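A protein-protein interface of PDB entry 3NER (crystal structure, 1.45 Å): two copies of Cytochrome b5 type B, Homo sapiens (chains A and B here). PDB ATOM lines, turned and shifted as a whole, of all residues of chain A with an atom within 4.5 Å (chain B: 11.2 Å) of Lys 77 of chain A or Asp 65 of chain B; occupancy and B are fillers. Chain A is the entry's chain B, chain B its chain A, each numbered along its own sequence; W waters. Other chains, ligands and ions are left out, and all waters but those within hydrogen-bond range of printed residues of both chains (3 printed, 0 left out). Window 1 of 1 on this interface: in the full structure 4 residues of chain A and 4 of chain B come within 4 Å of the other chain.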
ATOM      1  N   ARG A  33     -11.604  -3.413 -24.127  1.00  0.00           N
ATOM      2  CA  ARG A  33     -11.314  -2.279 -23.232  1.00  0.00           C
ATOM      3  C   ARG A  33     -10.919  -2.788 -21.865  1.00  0.00           C
ATOM      4  O   ARG A  33     -11.261  -3.914 -21.488  1.00  0.00           O
ATOM      5  CB  ARG A  33     -12.535  -1.397 -23.118  1.00  0.00           C
ATOM      6  CG  ARG A  33     -12.720  -0.655 -24.448  1.00  0.00           C
ATOM      7  CD  ARG A  33     -13.880   0.362 -24.322  1.00  0.00           C
ATOM      8  NE  ARG A  33     -13.596   1.469 -25.235  1.00  0.00           N
ATOM      9  CZ  ARG A  33     -14.427   2.499 -25.384  1.00  0.00           C
ATOM     10  NH1 ARG A  33     -15.549   2.523 -24.688  1.00  0.00           N
ATOM     11  NH2 ARG A  33     -14.095   3.499 -26.176  1.00  0.00           N
ATOM     12  N   ARG A  73     -24.370  -1.991 -17.709  1.00  0.00           N
ATOM     13  CA  ARG A  73     -23.492  -1.566 -18.830  1.00  0.00           C
ATOM     14  C   ARG A  73     -23.095  -0.079 -18.729  1.00  0.00           C
ATOM     15  O   ARG A  73     -21.964   0.350 -19.086  1.00  0.00           O
ATOM     16  CB  ARG A  73     -24.164  -1.857 -20.170  1.00  0.00           C
ATOM     17  CG  ARG A  73     -23.855  -3.240 -20.742  1.00  0.00           C
ATOM     18  CD  ARG A  73     -24.175  -3.231 -22.240  1.00  0.00           C
ATOM     19  NE  ARG A  73     -25.613  -3.208 -22.419  1.00  0.00           N
ATOM     20  CZ  ARG A  73     -26.388  -4.205 -22.029  1.00  0.00           C
ATOM     21  NH1 ARG A  73     -25.827  -5.276 -21.491  1.00  0.00           N
ATOM     22  NH2 ARG A  73     -27.705  -4.126 -22.136  1.00  0.00           N
ATOM     23  N   GLU A  74     -23.993   0.751 -18.244  1.00  0.00           N
ATOM     24  CA  GLU A  74     -23.642   2.137 -18.085  1.00  0.00           C
ATOM     25  C   GLU A  74     -22.624   2.286 -16.974  1.00  0.00           C
ATOM     26  O   GLU A  74     -21.693   3.085 -17.058  1.00  0.00           O
ATOM     27  CB  GLU A  74     -24.885   2.968 -17.742  1.00  0.00           C
ATOM     28  CG  GLU A  74     -25.573   3.442 -18.970  1.00  0.00           C
ATOM     29  CD  GLU A  74     -24.641   4.317 -19.814  1.00  0.00           C
ATOM     30  OE1 GLU A  74     -24.308   5.460 -19.384  1.00  0.00           O
ATOM     31  OE2 GLU A  74     -24.236   3.839 -20.905  1.00  0.00           O
ATOM     32  N   MET A  75     -22.821   1.492 -15.930  1.00  0.00           N
ATOM     33  CA  MET A  75     -21.944   1.480 -14.762  1.00  0.00           C
ATOM     34  C   MET A  75     -20.535   1.040 -15.162  1.00  0.00           C
ATOM     35  O   MET A  75     -19.559   1.522 -14.579  1.00  0.00           O
ATOM     36  CB  MET A  75     -22.515   0.496 -13.722  1.00  0.00           C
ATOM     37  CG  MET A  75     -21.903   0.563 -12.378  1.00  0.00           C
ATOM     38  SD  MET A  75     -22.680  -0.808 -11.389  1.00  0.00           S
ATOM     39  CE  MET A  75     -24.385  -0.383 -11.680  1.00  0.00           C
ATOM     40  N   LEU A  76     -20.432   0.130 -16.118  1.00  0.00           N
ATOM     41  CA  LEU A  76     -19.126  -0.360 -16.597  1.00  0.00           C
ATOM     42  C   LEU A  76     -18.254   0.821 -17.038  1.00  0.00           C
ATOM     43  O   LEU A  76     -17.057   0.873 -16.743  1.00  0.00           O
ATOM     44  CB  LEU A  76     -19.364  -1.335 -17.739  1.00  0.00           C
ATOM     45  CG  LEU A  76     -18.262  -2.047 -18.468  1.00  0.00           C
ATOM     46  CD1 LEU A  76     -17.381  -2.796 -17.535  1.00  0.00           C
ATOM     47  CD2 LEU A  76     -18.922  -2.974 -19.435  1.00  0.00           C
ATOM     48  N   LYS A  77     -18.853   1.812 -17.692  1.00  0.00           N
ATOM     49  CA  LYS A  77     -18.113   3.012 -18.107  1.00  0.00           C
ATOM     50  C   LYS A  77     -17.372   3.700 -16.966  1.00  0.00           C
ATOM     51  O   LYS A  77     -16.346   4.281 -17.206  1.00  0.00           O
ATOM     52  CB  LYS A  77     -19.047   4.028 -18.747  1.00  0.00           C
ATOM     53  CG  LYS A  77     -19.658   3.459 -20.032  1.00  0.00           C
ATOM     54  CD  LYS A  77     -20.464   4.512 -20.736  1.00  0.00           C
ATOM     55  CE  LYS A  77     -21.109   3.889 -21.977  1.00  0.00           C
ATOM     56  NZ  LYS A  77     -21.942   4.970 -22.630  1.00  0.00           N
ATOM     57  N   GLN A  78     -17.868   3.665 -15.739  1.00  0.00           N
ATOM     58  CA  GLN A  78     -17.162   4.319 -14.642  1.00  0.00           C
ATOM     59  C   GLN A  78     -15.820   3.694 -14.344  1.00  0.00           C
ATOM     60  O   GLN A  78     -14.948   4.325 -13.751  1.00  0.00           O
ATOM     61  CB  GLN A  78     -17.983   4.248 -13.318  1.00  0.00           C
ATOM     62  CG  GLN A  78     -19.364   4.861 -13.367  1.00  0.00           C
ATOM     63  CD  GLN A  78     -20.243   4.340 -12.253  1.00  0.00           C
ATOM     64  OE1 GLN A  78     -19.760   3.708 -11.306  1.00  0.00           O
ATOM     65  NE2 GLN A  78     -21.561   4.587 -12.371  1.00  0.00           N
ATOM     66  N   TYR A  79     -15.650   2.444 -14.737  1.00  0.00           N
ATOM     67  CA  TYR A  79     -14.405   1.726 -14.444  1.00  0.00           C
ATOM     68  C   TYR A  79     -13.426   1.664 -15.594  1.00  0.00           C
ATOM     69  O   TYR A  79     -12.344   1.144 -15.462  1.00  0.00           O
ATOM     70  CB  TYR A  79     -14.793   0.297 -13.963  1.00  0.00           C
ATOM     71  CG  TYR A  79     -15.647   0.407 -12.731  1.00  0.00           C
ATOM     72  CD1 TYR A  79     -15.117   0.758 -11.528  1.00  0.00           C
ATOM     73  CD2 TYR A  79     -16.995   0.251 -12.817  1.00  0.00           C
ATOM     74  CE1 TYR A  79     -15.935   0.943 -10.417  1.00  0.00           C
ATOM     75  CE2 TYR A  79     -17.805   0.478 -11.730  1.00  0.00           C
ATOM     76  CZ  TYR A  79     -17.276   0.806 -10.561  1.00  0.00           C
ATOM     77  OH  TYR A  79     -18.144   0.978  -9.504  1.00  0.00           O
ATOM     78  N   TYR A  80     -13.797   2.257 -16.700  1.00  0.00           N
ATOM     79  CA  TYR A  80     -12.933   2.256 -17.889  1.00  0.00           C
ATOM     80  C   TYR A  80     -11.643   2.973 -17.619  1.00  0.00           C
ATOM     81  O   TYR A  80     -11.649   4.130 -17.059  1.00  0.00           O
ATOM     82  CB  TYR A  80     -13.630   3.018 -18.999  1.00  0.00           C
ATOM     83  CG  TYR A  80     -12.812   3.242 -20.243  1.00  0.00           C
ATOM     84  CD1 TYR A  80     -12.715   2.245 -21.225  1.00  0.00           C
ATOM     85  CD2 TYR A  80     -12.098   4.438 -20.416  1.00  0.00           C
ATOM     86  CE1 TYR A  80     -11.913   2.447 -22.371  1.00  0.00           C
ATOM     87  CE2 TYR A  80     -11.291   4.653 -21.543  1.00  0.00           C
ATOM     88  CZ  TYR A  80     -11.221   3.653 -22.513  1.00  0.00           C
ATOM     89  OH  TYR A  80     -10.467   3.887 -23.660  1.00  0.00           O
ATOM     90  N   ILE B  30     -29.022   9.243 -34.092  1.00  0.00           N
ATOM     91  CA  ILE B  30     -27.626   9.578 -33.844  1.00  0.00           C
ATOM     92  C   ILE B  30     -27.361  10.916 -34.537  1.00  0.00           C
ATOM     93  O   ILE B  30     -27.601  11.107 -35.714  1.00  0.00           O
ATOM     94  CB  ILE B  30     -26.747   8.514 -34.461  1.00  0.00           C
ATOM     95  CG1 ILE B  30     -27.040   7.181 -33.745  1.00  0.00           C
ATOM     96  CG2 ILE B  30     -25.267   8.855 -34.305  1.00  0.00           C
ATOM     97  CD1 ILE B  30     -26.284   6.015 -34.400  1.00  0.00           C
ATOM     98  N   HIS B  31     -26.881  11.862 -33.750  1.00  0.00           N
ATOM     99  CA  HIS B  31     -26.572  13.216 -34.208  1.00  0.00           C
ATOM    100  C   HIS B  31     -27.653  13.832 -35.038  1.00  0.00           C
ATOM    101  O   HIS B  31     -27.385  14.360 -36.120  1.00  0.00           O
ATOM    102  CB  HIS B  31     -25.220  13.242 -34.937  1.00  0.00           C
ATOM    103  CG  HIS B  31     -24.091  12.761 -34.066  1.00  0.00           C
ATOM    104  ND1 HIS B  31     -23.856  13.237 -32.798  1.00  0.00           N
ATOM    105  CD2 HIS B  31     -23.161  11.807 -34.290  1.00  0.00           C
ATOM    106  CE1 HIS B  31     -22.829  12.584 -32.273  1.00  0.00           C
ATOM    107  NE2 HIS B  31     -22.387  11.716 -33.156  1.00  0.00           N
ATOM    108  N   HIS B  44     -24.126  -6.358 -36.458  1.00  0.00           N
ATOM    109  CA  HIS B  44     -23.410  -5.398 -35.636  1.00  0.00           C
ATOM    110  C   HIS B  44     -22.356  -6.034 -34.736  1.00  0.00           C
ATOM    111  O   HIS B  44     -22.650  -6.872 -33.907  1.00  0.00           O
ATOM    112  CB  HIS B  44     -24.388  -4.628 -34.741  1.00  0.00           C
ATOM    113  CG  HIS B  44     -23.716  -3.593 -33.910  1.00  0.00           C
ATOM    114  ND1 HIS B  44     -23.926  -3.498 -32.563  1.00  0.00           N
ATOM    115  CD2 HIS B  44     -22.863  -2.600 -34.230  1.00  0.00           C
ATOM    116  CE1 HIS B  44     -23.231  -2.484 -32.075  1.00  0.00           C
ATOM    117  NE2 HIS B  44     -22.573  -1.919 -33.062  1.00  0.00           N
ATOM    118  N   VAL B  50     -27.156  -3.785 -27.358  1.00  0.00           N
ATOM    119  CA  VAL B  50     -26.701  -2.413 -27.149  1.00  0.00           C
ATOM    120  C   VAL B  50     -27.398  -1.468 -28.117  1.00  0.00           C
ATOM    121  O   VAL B  50     -27.501  -0.277 -27.818  1.00  0.00           O
ATOM    122  CB  VAL B  50     -25.135  -2.243 -27.301  1.00  0.00           C
ATOM    123  CG1 VAL B  50     -24.425  -3.061 -26.239  1.00  0.00           C
ATOM    124  CG2 VAL B  50     -24.679  -2.597 -28.714  1.00  0.00           C
ATOM    125  N   GLU B  53     -31.470  -1.336 -26.833  1.00  0.00           N
ATOM    126  CA  GLU B  53     -31.751  -0.584 -25.606  1.00  0.00           C
ATOM    127  C   GLU B  53     -31.738   0.907 -25.784  1.00  0.00           C
ATOM    128  O   GLU B  53     -32.154   1.649 -24.894  1.00  0.00           O
ATOM    129  CB  GLU B  53     -30.795  -1.015 -24.489  1.00  0.00           C
ATOM    130  CG  GLU B  53     -29.386  -0.588 -24.615  1.00  0.00           C
ATOM    131  CD  GLU B  53     -28.456  -1.241 -23.544  1.00  0.00           C
ATOM    132  OE1 GLU B  53     -28.929  -2.072 -22.698  1.00  0.00           O
ATOM    133  OE2 GLU B  53     -27.267  -0.885 -23.567  1.00  0.00           O
ATOM    134  N   GLN B  54     -31.315   1.394 -26.952  1.00  0.00           N
ATOM    135  CA  GLN B  54     -31.334   2.829 -27.178  1.00  0.00           C
ATOM    136  C   GLN B  54     -32.548   3.259 -28.020  1.00  0.00           C
ATOM    137  O   GLN B  54     -32.628   4.380 -28.517  1.00  0.00           O
ATOM    138  CB  GLN B  54     -30.034   3.231 -27.915  1.00  0.00           C
ATOM    139  CG  GLN B  54     -28.792   2.941 -27.058  1.00  0.00           C
ATOM    140  CD  GLN B  54     -28.764   3.616 -25.655  1.00  0.00           C
ATOM    141  OE1 GLN B  54     -28.200   3.063 -24.674  1.00  0.00           O
ATOM    142  NE2 GLN B  54     -29.333   4.815 -25.571  1.00  0.00           N
ATOM    143  N   VAL B  57     -34.671   7.030 -27.812  1.00  0.00           N
ATOM    144  CA  VAL B  57     -33.958   8.090 -27.092  1.00  0.00           C
ATOM    145  C   VAL B  57     -32.790   8.524 -27.969  1.00  0.00           C
ATOM    146  O   VAL B  57     -32.600   8.034 -29.065  1.00  0.00           O
ATOM    147  CB  VAL B  57     -33.466   7.576 -25.683  1.00  0.00           C
ATOM    148  CG1 VAL B  57     -34.684   7.166 -24.820  1.00  0.00           C
ATOM    149  CG2 VAL B  57     -32.559   6.346 -25.825  1.00  0.00           C
ATOM    150  N   ASP B  58     -32.022   9.484 -27.519  1.00  0.00           N
ATOM    151  CA  ASP B  58     -30.876   9.892 -28.308  1.00  0.00           C
ATOM    152  C   ASP B  58     -29.726   8.909 -28.070  1.00  0.00           C
ATOM    153  O   ASP B  58     -29.245   8.778 -26.931  1.00  0.00           O
ATOM    154  CB  ASP B  58     -30.508  11.307 -27.868  1.00  0.00           C
ATOM    155  CG  ASP B  58     -29.474  11.953 -28.786  1.00  0.00           C
ATOM    156  OD1 ASP B  58     -28.858  11.275 -29.624  1.00  0.00           O
ATOM    157  OD2 ASP B  58     -29.281  13.193 -28.686  1.00  0.00           O
ATOM    158  N   ALA B  59     -29.249   8.259 -29.114  1.00  0.00           N
ATOM    159  CA  ALA B  59     -28.212   7.236 -29.016  1.00  0.00           C
ATOM    160  C   ALA B  59     -26.835   7.814 -29.274  1.00  0.00           C
ATOM    161  O   ALA B  59     -25.833   7.090 -29.248  1.00  0.00           O
ATOM    162  CB  ALA B  59     -28.531   6.145 -30.053  1.00  0.00           C
ATOM    163  N   SER B  60     -26.736   9.133 -29.438  1.00  0.00           N
ATOM    164  CA  SER B  60     -25.466   9.728 -29.856  1.00  0.00           C
ATOM    165  C   SER B  60     -24.359   9.504 -28.839  1.00  0.00           C
ATOM    166  O   SER B  60     -23.260   9.139 -29.246  1.00  0.00           O
ATOM    167  CB  SER B  60     -25.605  11.238 -30.064  1.00  0.00           C
ATOM    168  OG  SER B  60     -26.649  11.518 -31.003  1.00  0.00           O
ATOM    169  N   GLU B  61     -24.629   9.792 -27.558  1.00  0.00           N
ATOM    170  CA  GLU B  61     -23.615   9.611 -26.527  1.00  0.00           C
ATOM    171  C   GLU B  61     -23.159   8.144 -26.511  1.00  0.00           C
ATOM    172  O   GLU B  61     -21.973   7.874 -26.483  1.00  0.00           O
ATOM    173  CB  GLU B  61     -24.165   9.976 -25.143  1.00  0.00           C
ATOM    174  CG  GLU B  61     -23.061  10.196 -24.122  1.00  0.00           C
ATOM    175  CD  GLU B  61     -23.572  10.486 -22.698  1.00  0.00           C
ATOM    176  OE1 GLU B  61     -24.797  10.381 -22.456  1.00  0.00           O
ATOM    177  OE2 GLU B  61     -22.729  10.802 -21.809  1.00  0.00           O
ATOM    178  N   SER B  62     -24.121   7.212 -26.550  1.00  0.00           N
ATOM    179  CA  SER B  62     -23.758   5.797 -26.546  1.00  0.00           C
ATOM    180  C   SER B  62     -22.855   5.443 -27.705  1.00  0.00           C
ATOM    181  O   SER B  62     -21.879   4.678 -27.539  1.00  0.00           O
ATOM    182  CB  SER B  62     -25.013   4.904 -26.608  1.00  0.00           C
ATOM    183  OG  SER B  62     -25.832   5.163 -25.491  1.00  0.00           O
ATOM    184  N   PHE B  63     -23.197   5.926 -28.892  1.00  0.00           N
ATOM    185  CA  PHE B  63     -22.436   5.679 -30.084  1.00  0.00           C
ATOM    186  C   PHE B  63     -21.035   6.283 -29.989  1.00  0.00           C
ATOM    187  O   PHE B  63     -20.043   5.667 -30.368  1.00  0.00           O
ATOM    188  CB  PHE B  63     -23.206   6.292 -31.282  1.00  0.00           C
ATOM    189  CG  PHE B  63     -22.557   6.050 -32.608  1.00  0.00           C
ATOM    190  CD1 PHE B  63     -22.679   4.814 -33.279  1.00  0.00           C
ATOM    191  CD2 PHE B  63     -21.764   7.049 -33.197  1.00  0.00           C
ATOM    192  CE1 PHE B  63     -22.015   4.568 -34.533  1.00  0.00           C
ATOM    193  CE2 PHE B  63     -21.124   6.833 -34.428  1.00  0.00           C
ATOM    194  CZ  PHE B  63     -21.237   5.592 -35.106  1.00  0.00           C
ATOM    195  N   GLU B  64     -20.944   7.514 -29.491  1.00  0.00           N
ATOM    196  CA  GLU B  64     -19.634   8.155 -29.453  1.00  0.00           C
ATOM    197  C   GLU B  64     -18.727   7.560 -28.379  1.00  0.00           C
ATOM    198  O   GLU B  64     -17.505   7.475 -28.599  1.00  0.00           O
ATOM    199  CB  GLU B  64     -19.792   9.654 -29.233  1.00  0.00           C
ATOM    200  CG  GLU B  64     -20.410  10.351 -30.441  1.00  0.00           C
ATOM    201  CD  GLU B  64     -19.540  10.256 -31.692  1.00  0.00           C
ATOM    202  OE1 GLU B  64     -18.287  10.122 -31.580  1.00  0.00           O
ATOM    203  OE2 GLU B  64     -20.115  10.286 -32.817  1.00  0.00           O
ATOM    204  N   ASP B  65     -19.299   7.132 -27.259  1.00  0.00           N
ATOM    205  CA  ASP B  65     -18.477   6.596 -26.157  1.00  0.00           C
ATOM    206  C   ASP B  65     -17.753   5.313 -26.567  1.00  0.00           C
ATOM    207  O   ASP B  65     -16.652   5.019 -26.064  1.00  0.00           O
ATOM    208  CB  ASP B  65     -19.330   6.289 -24.926  1.00  0.00           C
ATOM    209  CG  ASP B  65     -19.750   7.519 -24.160  1.00  0.00           C
ATOM    210  OD1 ASP B  65     -19.184   8.609 -24.352  1.00  0.00           O
ATOM    211  OD2 ASP B  65     -20.659   7.390 -23.328  1.00  0.00           O
ATOM    212  N   VAL B  66     -18.326   4.572 -27.491  1.00  0.00           N
ATOM    213  CA  VAL B  66     -17.707   3.312 -27.928  1.00  0.00           C
ATOM    214  C   VAL B  66     -16.427   3.543 -28.722  1.00  0.00           C
ATOM    215  O   VAL B  66     -15.596   2.648 -28.811  1.00  0.00           O
ATOM    216  CB  VAL B  66     -18.750   2.537 -28.781  1.00  0.00           C
ATOM    217  CG1 VAL B  66     -18.064   1.560 -29.736  1.00  0.00           C
ATOM    218  CG2 VAL B  66     -19.717   1.882 -27.889  1.00  0.00           C
ATOM    219  N   GLY B  67     -16.268   4.703 -29.352  1.00  0.00           N
ATOM    220  CA  GLY B  67     -15.069   4.908 -30.177  1.00  0.00           C
ATOM    221  C   GLY B  67     -15.146   4.127 -31.487  1.00  0.00           C
ATOM    222  O   GLY B  67     -14.249   3.345 -31.863  1.00  0.00           O
ATOM    223  N   HIS B  68     -16.258   4.315 -32.180  1.00  0.00           N
ATOM    224  CA  HIS B  68     -16.482   3.660 -33.467  1.00  0.00           C
ATOM    225  C   HIS B  68     -15.477   4.168 -34.489  1.00  0.00           C
ATOM    226  O   HIS B  68     -15.190   5.353 -34.535  1.00  0.00           O
ATOM    227  CB  HIS B  68     -17.907   3.985 -33.980  1.00  0.00           C
ATOM    228  CG  HIS B  68     -18.982   3.111 -33.415  1.00  0.00           C
ATOM    229  ND1 HIS B  68     -19.706   3.449 -32.289  1.00  0.00           N
ATOM    230  CD2 HIS B  68     -19.400   1.884 -33.781  1.00  0.00           C
ATOM    231  CE1 HIS B  68     -20.524   2.458 -31.985  1.00  0.00           C
ATOM    232  NE2 HIS B  68     -20.360   1.482 -32.877  1.00  0.00           N
ATOM    233  N   SER B  69     -14.975   3.254 -35.299  1.00  0.00           N
ATOM    234  CA  SER B  69     -13.975   3.556 -36.340  1.00  0.00           C
ATOM    235  C   SER B  69     -14.564   4.400 -37.473  1.00  0.00           C
ATOM    236  O   SER B  69     -15.778   4.644 -37.566  1.00  0.00           O
ATOM    237  CB  SER B  69     -13.469   2.249 -36.928  1.00  0.00           C
ATOM    238  OG  SER B  69     -14.497   1.640 -37.721  1.00  0.00           O
ATOM    239  N   ALA B  72     -16.870   2.326 -39.386  1.00  0.00           N
ATOM    240  CA  ALA B  72     -18.196   2.208 -38.778  1.00  0.00           C
ATOM    241  C   ALA B  72     -19.040   3.442 -39.101  1.00  0.00           C
ATOM    242  O   ALA B  72     -20.236   3.336 -39.337  1.00  0.00           O
ATOM    243  CB  ALA B  72     -18.070   2.074 -37.255  1.00  0.00           C
ATOM    244  N   ARG B  73     -18.437   4.617 -39.066  1.00  0.00           N
ATOM    245  CA  ARG B  73     -19.138   5.864 -39.351  1.00  0.00           C
ATOM    246  C   ARG B  73     -19.604   5.958 -40.769  1.00  0.00           C
ATOM    247  O   ARG B  73     -20.676   6.489 -41.060  1.00  0.00           O
ATOM    248  CB  ARG B  73     -18.241   7.066 -39.022  1.00  0.00           C
ATOM    249  CG  ARG B  73     -18.033   7.239 -37.516  1.00  0.00           C
ATOM    250  CD  ARG B  73     -17.126   8.468 -37.163  1.00  0.00           C
ATOM    251  NE  ARG B  73     -16.780   8.354 -35.753  1.00  0.00           N
ATOM    252  CZ  ARG B  73     -17.543   8.809 -34.754  1.00  0.00           C
ATOM    253  NH1 ARG B  73     -18.670   9.458 -35.012  1.00  0.00           N
ATOM    254  NH2 ARG B  73     -17.188   8.567 -33.495  1.00  0.00           N
HETATM  255  O   HOH W   1     -21.700   3.379 -25.125  1.00  0.00           O
HETATM  256  O   HOH W   2     -31.200  -4.180 -22.235  1.00  0.00           O
HETATM  257  O   HOH W   3     -24.967   4.008 -23.340  1.00  0.00           O
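Water W3 lies within hydrogen-bond range of OE2 of Glu 74 of chain A (2.5 Å), OG of Ser 62 of chain B (2.6 Å) and NZ of Lys 77 of chain A (3.3 Å). Water W1 bridges O of Ser 62 of chain B (2.7 Å) and NZ of Lys 77 of chain A (3.0 Å). Water W2 lies within hydrogen-bond range of OE1 of Glu 53 of chain B (3.1 Å) and NH2 of Arg 73 of chain A (3.5 Å).
Printed residues of chain B within 4 Å of Arg 33 of chain A: Asp 65 and Val 66. Printed residues of chain B within 4 Å of Arg 73 of chain A: Glu 53. No residue of chain B comes within 4 Å of Glu 74 of chain A. No residue of chain B comes within 4 Å of Leu 76 of chain A. Lys 77 of chain A touches just one residue of chain B: Asp 65. No residue of chain B comes within 4 Å of Gln 78 of chain A. No residue of chain B comes within 4 Å of Tyr 80 of chain A. Of the printed residues of chain A, Glu 53 of chain B touches Arg 73. Asp 65 of chain B touches two residues of chain A. Of the printed residues of chain A, Val 66 of chain B touches Arg 33 (3.1 Å). The nearest residue of chain B that does not touch Lys 77 of chain A is Ser 62 of chain B (4.4 Å).
Position printed for both chains: 73. Of the 4 pairs that touch across the chains among the printed residues, none has its exchanged pair printed and touching as well.
Of the 9 printed residues of chain A, 3 touch a printed residue of chain B. Of the 21 printed residues of chain B, 3 touch a printed residue of chain A. Among the printed residues, 4 pairs touch across the chains. Among the printed residues, Asp or Glu carboxylates within 4 Å of a Lys or Arg side-chain nitrogen of the other chain: Arg 73 of chain A with Glu 53 of chain B and Lys 77 of chain A with Asp 65 of chain B.
The side-chain carboxylate (OE2) of Glu 74 of chain A is in salt-bridge range of the side-chain amino group (NZ) of Lys 77 of chain A (3.1 Å).
The side-chain carboxylate (OE1) of Glu 53 of chain B lies within salt-bridge range of the guanidinium group (NH2) of Arg 73 of chain A (2.5 Å). NH2 of Arg 33 of chain A is in hydrogen-bond range of O of Asp 65 of chain B, 3.0 Å away. The side-chain carboxylate (OD2) of Asp 65 of chain B is in salt-bridge range of the side-chain amino group (NZ) of Lys 77 of chain A, at 2.8 Å. The backbone carbonyl oxygen (O) of Val 66 of chain B is in hydrogen-bond range of the guanidinium group (NH2) of Arg 33 of chain A.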
